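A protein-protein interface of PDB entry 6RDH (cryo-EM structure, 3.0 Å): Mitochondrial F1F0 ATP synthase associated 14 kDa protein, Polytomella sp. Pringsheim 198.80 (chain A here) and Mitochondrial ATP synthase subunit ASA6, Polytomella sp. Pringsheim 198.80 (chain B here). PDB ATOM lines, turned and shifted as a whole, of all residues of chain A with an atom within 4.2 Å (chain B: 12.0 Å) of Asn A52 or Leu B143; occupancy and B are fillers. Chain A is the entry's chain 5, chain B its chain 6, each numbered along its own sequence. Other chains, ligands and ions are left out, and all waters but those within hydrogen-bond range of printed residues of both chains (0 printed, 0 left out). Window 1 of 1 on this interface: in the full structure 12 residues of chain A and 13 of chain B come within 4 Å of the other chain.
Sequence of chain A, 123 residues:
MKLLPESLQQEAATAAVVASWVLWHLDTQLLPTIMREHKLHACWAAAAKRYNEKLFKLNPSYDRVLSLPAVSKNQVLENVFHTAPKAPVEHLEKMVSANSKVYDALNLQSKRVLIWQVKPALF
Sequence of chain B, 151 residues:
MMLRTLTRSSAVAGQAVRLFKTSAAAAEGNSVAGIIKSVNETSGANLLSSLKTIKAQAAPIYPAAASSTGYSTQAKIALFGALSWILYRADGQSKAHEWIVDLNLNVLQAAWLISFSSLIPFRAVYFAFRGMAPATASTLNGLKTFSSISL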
ATOM      1  N   ALA A  48      20.976   4.698  29.267  1.00  0.00           N
ATOM      2  CA  ALA A  48      21.368   5.716  28.293  1.00  0.00           C
ATOM      3  C   ALA A  48      20.417   5.845  27.113  1.00  0.00           C
ATOM      4  O   ALA A  48      20.037   6.958  26.745  1.00  0.00           O
ATOM      5  CB  ALA A  48      22.769   5.402  27.791  1.00  0.00           C
ATOM      6  N   LYS A  49      19.966   4.721  26.561  1.00  0.00           N
ATOM      7  CA  LYS A  49      19.095   4.749  25.390  1.00  0.00           C
ATOM      8  C   LYS A  49      17.720   5.315  25.726  1.00  0.00           C
ATOM      9  O   LYS A  49      17.242   6.242  25.065  1.00  0.00           O
ATOM     10  CB  LYS A  49      18.983   3.340  24.814  1.00  0.00           C
ATOM     11  CG  LYS A  49      18.448   3.261  23.409  1.00  0.00           C
ATOM     12  CD  LYS A  49      17.014   2.769  23.413  1.00  0.00           C
ATOM     13  CE  LYS A  49      16.317   3.078  22.104  1.00  0.00           C
ATOM     14  NZ  LYS A  49      14.840   3.145  22.271  1.00  0.00           N
ATOM     15  N   ARG A  50      17.086   4.791  26.772  1.00  0.00           N
ATOM     16  CA  ARG A  50      15.756   5.253  27.151  1.00  0.00           C
ATOM     17  C   ARG A  50      15.789   6.641  27.763  1.00  0.00           C
ATOM     18  O   ARG A  50      14.846   7.413  27.586  1.00  0.00           O
ATOM     19  CB  ARG A  50      15.125   4.266  28.122  1.00  0.00           C
ATOM     20  CG  ARG A  50      14.738   2.965  27.469  1.00  0.00           C
ATOM     21  CD  ARG A  50      14.208   1.973  28.469  1.00  0.00           C
ATOM     22  NE  ARG A  50      13.374   2.596  29.485  1.00  0.00           N
ATOM     23  CZ  ARG A  50      12.519   1.919  30.235  1.00  0.00           C
ATOM     24  NH1 ARG A  50      11.792   2.539  31.152  1.00  0.00           N
ATOM     25  NH2 ARG A  50      12.392   0.612  30.059  1.00  0.00           N
ATOM     26  N   TYR A  51      16.868   6.971  28.463  1.00  0.00           N
ATOM     27  CA  TYR A  51      17.061   8.294  29.029  1.00  0.00           C
ATOM     28  C   TYR A  51      17.187   9.337  27.940  1.00  0.00           C
ATOM     29  O   TYR A  51      16.571  10.400  28.022  1.00  0.00           O
ATOM     30  CB  TYR A  51      18.311   8.277  29.899  1.00  0.00           C
ATOM     31  CG  TYR A  51      18.617   9.532  30.659  1.00  0.00           C
ATOM     32  CD1 TYR A  51      18.131   9.720  31.937  1.00  0.00           C
ATOM     33  CD2 TYR A  51      19.441  10.498  30.127  1.00  0.00           C
ATOM     34  CE1 TYR A  51      18.429  10.853  32.638  1.00  0.00           C
ATOM     35  CE2 TYR A  51      19.734  11.624  30.816  1.00  0.00           C
ATOM     36  CZ  TYR A  51      19.233  11.800  32.069  1.00  0.00           C
ATOM     37  OH  TYR A  51      19.539  12.937  32.757  1.00  0.00           O
ATOM     38  N   ASN A  52      17.966   9.044  26.901  1.00  0.00           N
ATOM     39  CA  ASN A  52      18.141  10.001  25.829  1.00  0.00           C
ATOM     40  C   ASN A  52      16.904  10.105  24.963  1.00  0.00           C
ATOM     41  O   ASN A  52      16.608  11.187  24.466  1.00  0.00           O
ATOM     42  CB  ASN A  52      19.345   9.616  24.997  1.00  0.00           C
ATOM     43  CG  ASN A  52      20.619   9.892  25.704  1.00  0.00           C
ATOM     44  OD1 ASN A  52      20.794  10.960  26.261  1.00  0.00           O
ATOM     45  ND2 ASN A  52      21.521   8.933  25.699  1.00  0.00           N
ATOM     46  N   GLU A  53      16.151   9.021  24.794  1.00  0.00           N
ATOM     47  CA  GLU A  53      14.892   9.147  24.068  1.00  0.00           C
ATOM     48  C   GLU A  53      13.866   9.940  24.864  1.00  0.00           C
ATOM     49  O   GLU A  53      13.147  10.766  24.299  1.00  0.00           O
ATOM     50  CB  GLU A  53      14.349   7.772  23.715  1.00  0.00           C
ATOM     51  CG  GLU A  53      13.118   7.814  22.842  1.00  0.00           C
ATOM     52  CD  GLU A  53      13.379   8.434  21.488  1.00  0.00           C
ATOM     53  OE1 GLU A  53      14.397   8.089  20.858  1.00  0.00           O
ATOM     54  OE2 GLU A  53      12.563   9.267  21.047  1.00  0.00           O
ATOM     55  N   LYS A  54      13.819   9.745  26.181  1.00  0.00           N
ATOM     56  CA  LYS A  54      12.895  10.499  27.021  1.00  0.00           C
ATOM     57  C   LYS A  54      13.273  11.972  27.084  1.00  0.00           C
ATOM     58  O   LYS A  54      12.402  12.846  27.096  1.00  0.00           O
ATOM     59  CB  LYS A  54      12.872   9.883  28.415  1.00  0.00           C
ATOM     60  CG  LYS A  54      11.898  10.505  29.372  1.00  0.00           C
ATOM     61  CD  LYS A  54      11.888   9.764  30.679  1.00  0.00           C
ATOM     62  CE  LYS A  54      10.795  10.290  31.574  1.00  0.00           C
ATOM     63  NZ  LYS A  54      10.694   9.550  32.855  1.00  0.00           N
ATOM     64  N   LEU A  55      14.565  12.271  27.087  1.00  0.00           N
ATOM     65  CA  LEU A  55      15.011  13.654  27.109  1.00  0.00           C
ATOM     66  C   LEU A  55      14.880  14.317  25.750  1.00  0.00           C
ATOM     67  O   LEU A  55      14.684  15.529  25.676  1.00  0.00           O
ATOM     68  CB  LEU A  55      16.454  13.716  27.595  1.00  0.00           C
ATOM     69  CG  LEU A  55      17.033  15.070  27.958  1.00  0.00           C
ATOM     70  CD1 LEU A  55      16.036  15.877  28.701  1.00  0.00           C
ATOM     71  CD2 LEU A  55      18.216  14.878  28.810  1.00  0.00           C
ATOM     72  N   PHE A  56      15.003  13.547  24.673  1.00  0.00           N
ATOM     73  CA  PHE A  56      14.699  14.047  23.342  1.00  0.00           C
ATOM     74  C   PHE A  56      13.232  14.420  23.233  1.00  0.00           C
ATOM     75  O   PHE A  56      12.888  15.476  22.699  1.00  0.00           O
ATOM     76  CB  PHE A  56      15.059  12.975  22.325  1.00  0.00           C
ATOM     77  CG  PHE A  56      15.100  13.445  20.919  1.00  0.00           C
ATOM     78  CD1 PHE A  56      16.100  14.280  20.489  1.00  0.00           C
ATOM     79  CD2 PHE A  56      14.170  12.999  20.008  1.00  0.00           C
ATOM     80  CE1 PHE A  56      16.154  14.686  19.188  1.00  0.00           C
ATOM     81  CE2 PHE A  56      14.223  13.411  18.709  1.00  0.00           C
ATOM     82  CZ  PHE A  56      15.215  14.253  18.298  1.00  0.00           C
ATOM     83  N   VAL B  32      25.429  26.737  37.375  1.00  0.00           N
ATOM     84  CA  VAL B  32      24.738  27.117  36.152  1.00  0.00           C
ATOM     85  C   VAL B  32      23.800  28.288  36.411  1.00  0.00           C
ATOM     86  O   VAL B  32      23.700  29.204  35.592  1.00  0.00           O
ATOM     87  CB  VAL B  32      24.017  25.898  35.564  1.00  0.00           C
ATOM     88  CG1 VAL B  32      23.153  26.286  34.433  1.00  0.00           C
ATOM     89  CG2 VAL B  32      25.032  24.942  35.056  1.00  0.00           C
ATOM     90  N   THR B 139      34.147   3.748  29.002  1.00  0.00           N
ATOM     91  CA  THR B 139      33.719   5.066  29.437  1.00  0.00           C
ATOM     92  C   THR B 139      32.222   5.080  29.728  1.00  0.00           C
ATOM     93  O   THR B 139      31.505   4.110  29.480  1.00  0.00           O
ATOM     94  CB  THR B 139      34.052   6.113  28.382  1.00  0.00           C
ATOM     95  OG1 THR B 139      33.776   5.576  27.084  1.00  0.00           O
ATOM     96  CG2 THR B 139      35.510   6.508  28.463  1.00  0.00           C
ATOM     97  N   LEU B 140      31.750   6.207  30.252  1.00  0.00           N
ATOM     98  CA  LEU B 140      30.338   6.368  30.553  1.00  0.00           C
ATOM     99  C   LEU B 140      29.527   6.499  29.267  1.00  0.00           C
ATOM    100  O   LEU B 140      30.068   6.662  28.172  1.00  0.00           O
ATOM    101  CB  LEU B 140      30.123   7.587  31.435  1.00  0.00           C
ATOM    102  CG  LEU B 140      30.071   7.356  32.929  1.00  0.00           C
ATOM    103  CD1 LEU B 140      29.637   8.611  33.548  1.00  0.00           C
ATOM    104  CD2 LEU B 140      29.086   6.292  33.244  1.00  0.00           C
ATOM    105  N   ASN B 141      28.203   6.444  29.398  1.00  0.00           N
ATOM    106  CA  ASN B 141      27.415   6.307  28.188  1.00  0.00           C
ATOM    107  C   ASN B 141      26.209   7.222  28.039  1.00  0.00           C
ATOM    108  O   ASN B 141      25.762   7.398  26.904  1.00  0.00           O
ATOM    109  CB  ASN B 141      26.939   4.866  28.044  1.00  0.00           C
ATOM    110  CG  ASN B 141      26.857   4.433  26.615  1.00  0.00           C
ATOM    111  OD1 ASN B 141      27.560   4.959  25.763  1.00  0.00           O
ATOM    112  ND2 ASN B 141      25.993   3.472  26.336  1.00  0.00           N
ATOM    113  N   GLY B 142      25.663   7.816  29.089  1.00  0.00           N
ATOM    114  CA  GLY B 142      24.444   8.585  28.930  1.00  0.00           C
ATOM    115  C   GLY B 142      24.666   9.942  28.293  1.00  0.00           C
ATOM    116  O   GLY B 142      25.778  10.304  27.922  1.00  0.00           O
ATOM    117  N   LEU B 143      23.559  10.667  28.114  1.00  0.00           N
ATOM    118  CA  LEU B 143      23.517  12.107  27.836  1.00  0.00           C
ATOM    119  C   LEU B 143      24.311  12.499  26.585  1.00  0.00           C
ATOM    120  O   LEU B 143      25.399  13.060  26.653  1.00  0.00           O
ATOM    121  CB  LEU B 143      23.957  12.918  29.050  1.00  0.00           C
ATOM    122  CG  LEU B 143      23.207  14.249  29.059  1.00  0.00           C
ATOM    123  CD1 LEU B 143      21.756  14.018  29.090  1.00  0.00           C
ATOM    124  CD2 LEU B 143      23.549  15.085  30.223  1.00  0.00           C
ATOM    125  N   LYS B 144      23.745  12.154  25.431  1.00  0.00           N
ATOM    126  CA  LYS B 144      24.469  12.188  24.169  1.00  0.00           C
ATOM    127  C   LYS B 144      24.403  13.533  23.455  1.00  0.00           C
ATOM    128  O   LYS B 144      24.391  13.553  22.215  1.00  0.00           O
ATOM    129  CB  LYS B 144      23.958  11.083  23.252  1.00  0.00           C
ATOM    130  CG  LYS B 144      24.469   9.727  23.612  1.00  0.00           C
ATOM    131  CD  LYS B 144      25.967   9.674  23.492  1.00  0.00           C
ATOM    132  CE  LYS B 144      26.474   8.288  23.825  1.00  0.00           C
ATOM    133  NZ  LYS B 144      27.956   8.201  23.755  1.00  0.00           N
ATOM    134  N   THR B 145      24.261  14.645  24.190  1.00  0.00           N
ATOM    135  CA  THR B 145      24.640  16.009  23.791  1.00  0.00           C
ATOM    136  C   THR B 145      23.701  16.620  22.744  1.00  0.00           C
ATOM    137  O   THR B 145      23.650  17.841  22.579  1.00  0.00           O
ATOM    138  CB  THR B 145      26.101  16.009  23.285  1.00  0.00           C
ATOM    139  OG1 THR B 145      26.920  15.304  24.223  1.00  0.00           O
ATOM    140  CG2 THR B 145      26.691  17.409  23.187  1.00  0.00           C
ATOM    141  N   PHE B 146      22.863  15.809  22.115  1.00  0.00           N
ATOM    142  CA  PHE B 146      21.792  16.301  21.269  1.00  0.00           C
ATOM    143  C   PHE B 146      20.456  16.292  21.970  1.00  0.00           C
ATOM    144  O   PHE B 146      19.560  17.035  21.569  1.00  0.00           O
ATOM    145  CB  PHE B 146      21.682  15.463  20.005  1.00  0.00           C
ATOM    146  CG  PHE B 146      22.198  16.133  18.781  1.00  0.00           C
ATOM    147  CD1 PHE B 146      21.341  16.822  17.952  1.00  0.00           C
ATOM    148  CD2 PHE B 146      23.534  16.095  18.463  1.00  0.00           C
ATOM    149  CE1 PHE B 146      21.808  17.427  16.816  1.00  0.00           C
ATOM    150  CE2 PHE B 146      24.001  16.702  17.332  1.00  0.00           C
ATOM    151  CZ  PHE B 146      23.140  17.373  16.513  1.00  0.00           C
ATOM    152  N   SER B 147      20.295  15.456  22.987  1.00  0.00           N
ATOM    153  CA  SER B 147      19.047  15.440  23.721  1.00  0.00           C
ATOM    154  C   SER B 147      18.956  16.604  24.683  1.00  0.00           C
ATOM    155  O   SER B 147      17.855  17.061  24.991  1.00  0.00           O
ATOM    156  CB  SER B 147      18.903  14.126  24.470  1.00  0.00           C
ATOM    157  OG  SER B 147      20.013  13.906  25.309  1.00  0.00           O
ATOM    158  N   SER B 148      20.089  17.120  25.135  1.00  0.00           N
ATOM    159  CA  SER B 148      20.076  18.107  26.199  1.00  0.00           C
ATOM    160  C   SER B 148      20.603  19.452  25.739  1.00  0.00           C
ATOM    161  O   SER B 148      21.415  20.066  26.433  1.00  0.00           O
ATOM    162  CB  SER B 148      20.898  17.615  27.379  1.00  0.00           C
ATOM    163  OG  SER B 148      22.247  17.465  26.996  1.00  0.00           O
ATOM    164  N   ILE B 149      20.169  19.918  24.584  1.00  0.00           N
ATOM    165  CA  ILE B 149      20.488  21.267  24.148  1.00  0.00           C
ATOM    166  C   ILE B 149      19.312  22.167  24.462  1.00  0.00           C
ATOM    167  O   ILE B 149      18.160  21.729  24.515  1.00  0.00           O
ATOM    168  CB  ILE B 149      20.829  21.347  22.655  1.00  0.00           C
ATOM    169  CG1 ILE B 149      19.780  20.610  21.869  1.00  0.00           C
ATOM    170  CG2 ILE B 149      22.189  20.781  22.371  1.00  0.00           C
ATOM    171  CD1 ILE B 149      19.976  20.788  20.458  1.00  0.00           C
ATOM    172  N   SER B 150      19.607  23.444  24.655  1.00  0.00           N
ATOM    173  CA  SER B 150      18.609  24.450  24.976  1.00  0.00           C
ATOM    174  C   SER B 150      18.737  25.555  23.938  1.00  0.00           C
ATOM    175  O   SER B 150      19.490  26.511  24.122  1.00  0.00           O
ATOM    176  CB  SER B 150      18.817  24.971  26.368  1.00  0.00           C
ATOM    177  OG  SER B 150      18.701  23.937  27.319  1.00  0.00           O
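OD1 of Asn A52 lies within hydrogen-bond range of OG of Ser B147 (3.2 Å). N of Leu B143 sits at hydrogen-bond distance from OD1 of Asn A52 (3.3 Å). The backbone NH of Lys B144 is in hydrogen-bond range of the side-chain amide oxygen of Asn A52, at 3.3 Å.
The side-chain amide nitrogen (ND2) of Asn A52 is in hydrogen-bond range of the backbone carbonyl oxygen (O) of Ala A48, at 2.7 Å.
Asn B141 touches Ala A48. Gly B142 touches Ala A48. Leu B143 touches Tyr A51. Leu A55 touches Leu B143. Ser B147 touches Leu A55 (O to O, 3.6 Å). Phe A56 touches Ser B147.
No residue of chain B comes within 4 Å of Lys A49. Of the printed residues of chain B, Asn A52 touches Leu B143 (3.3 Å), Lys B144 (3.3 Å) and Ser B147 (3.2 Å). No residue of chain B comes within 4 Å of Glu A53. Printed residues of chain A within 4 Å of Asn B141: Ala A48 (3.7 Å). Printed residues of chain A within 4 Å of Gly B142: Ala A48 (3.8 Å). Leu B143 touches just these residues of chain A: Tyr A51 (3.6 Å), Asn A52 (3.3 Å) and Leu A55 (3.7 Å). Printed residues of chain A within 4 Å of Lys B144: Asn A52 (3.3 Å). The nearest printed residue of chain A that does not touch Leu B143 is Ala A48 (5.3 Å). The nearest printed residue of chain A that does not touch Lys B144 is Ala A48 (6.1 Å).
Of the 9 printed residues of chain A, 5 touch a printed residue of chain B. Hydrophobic or aromatic side chains of chain A that line the printed part of chain B: Ala A48, Tyr A51 and Leu A55. Among the printed residues, 9 pairs touch across the chains.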
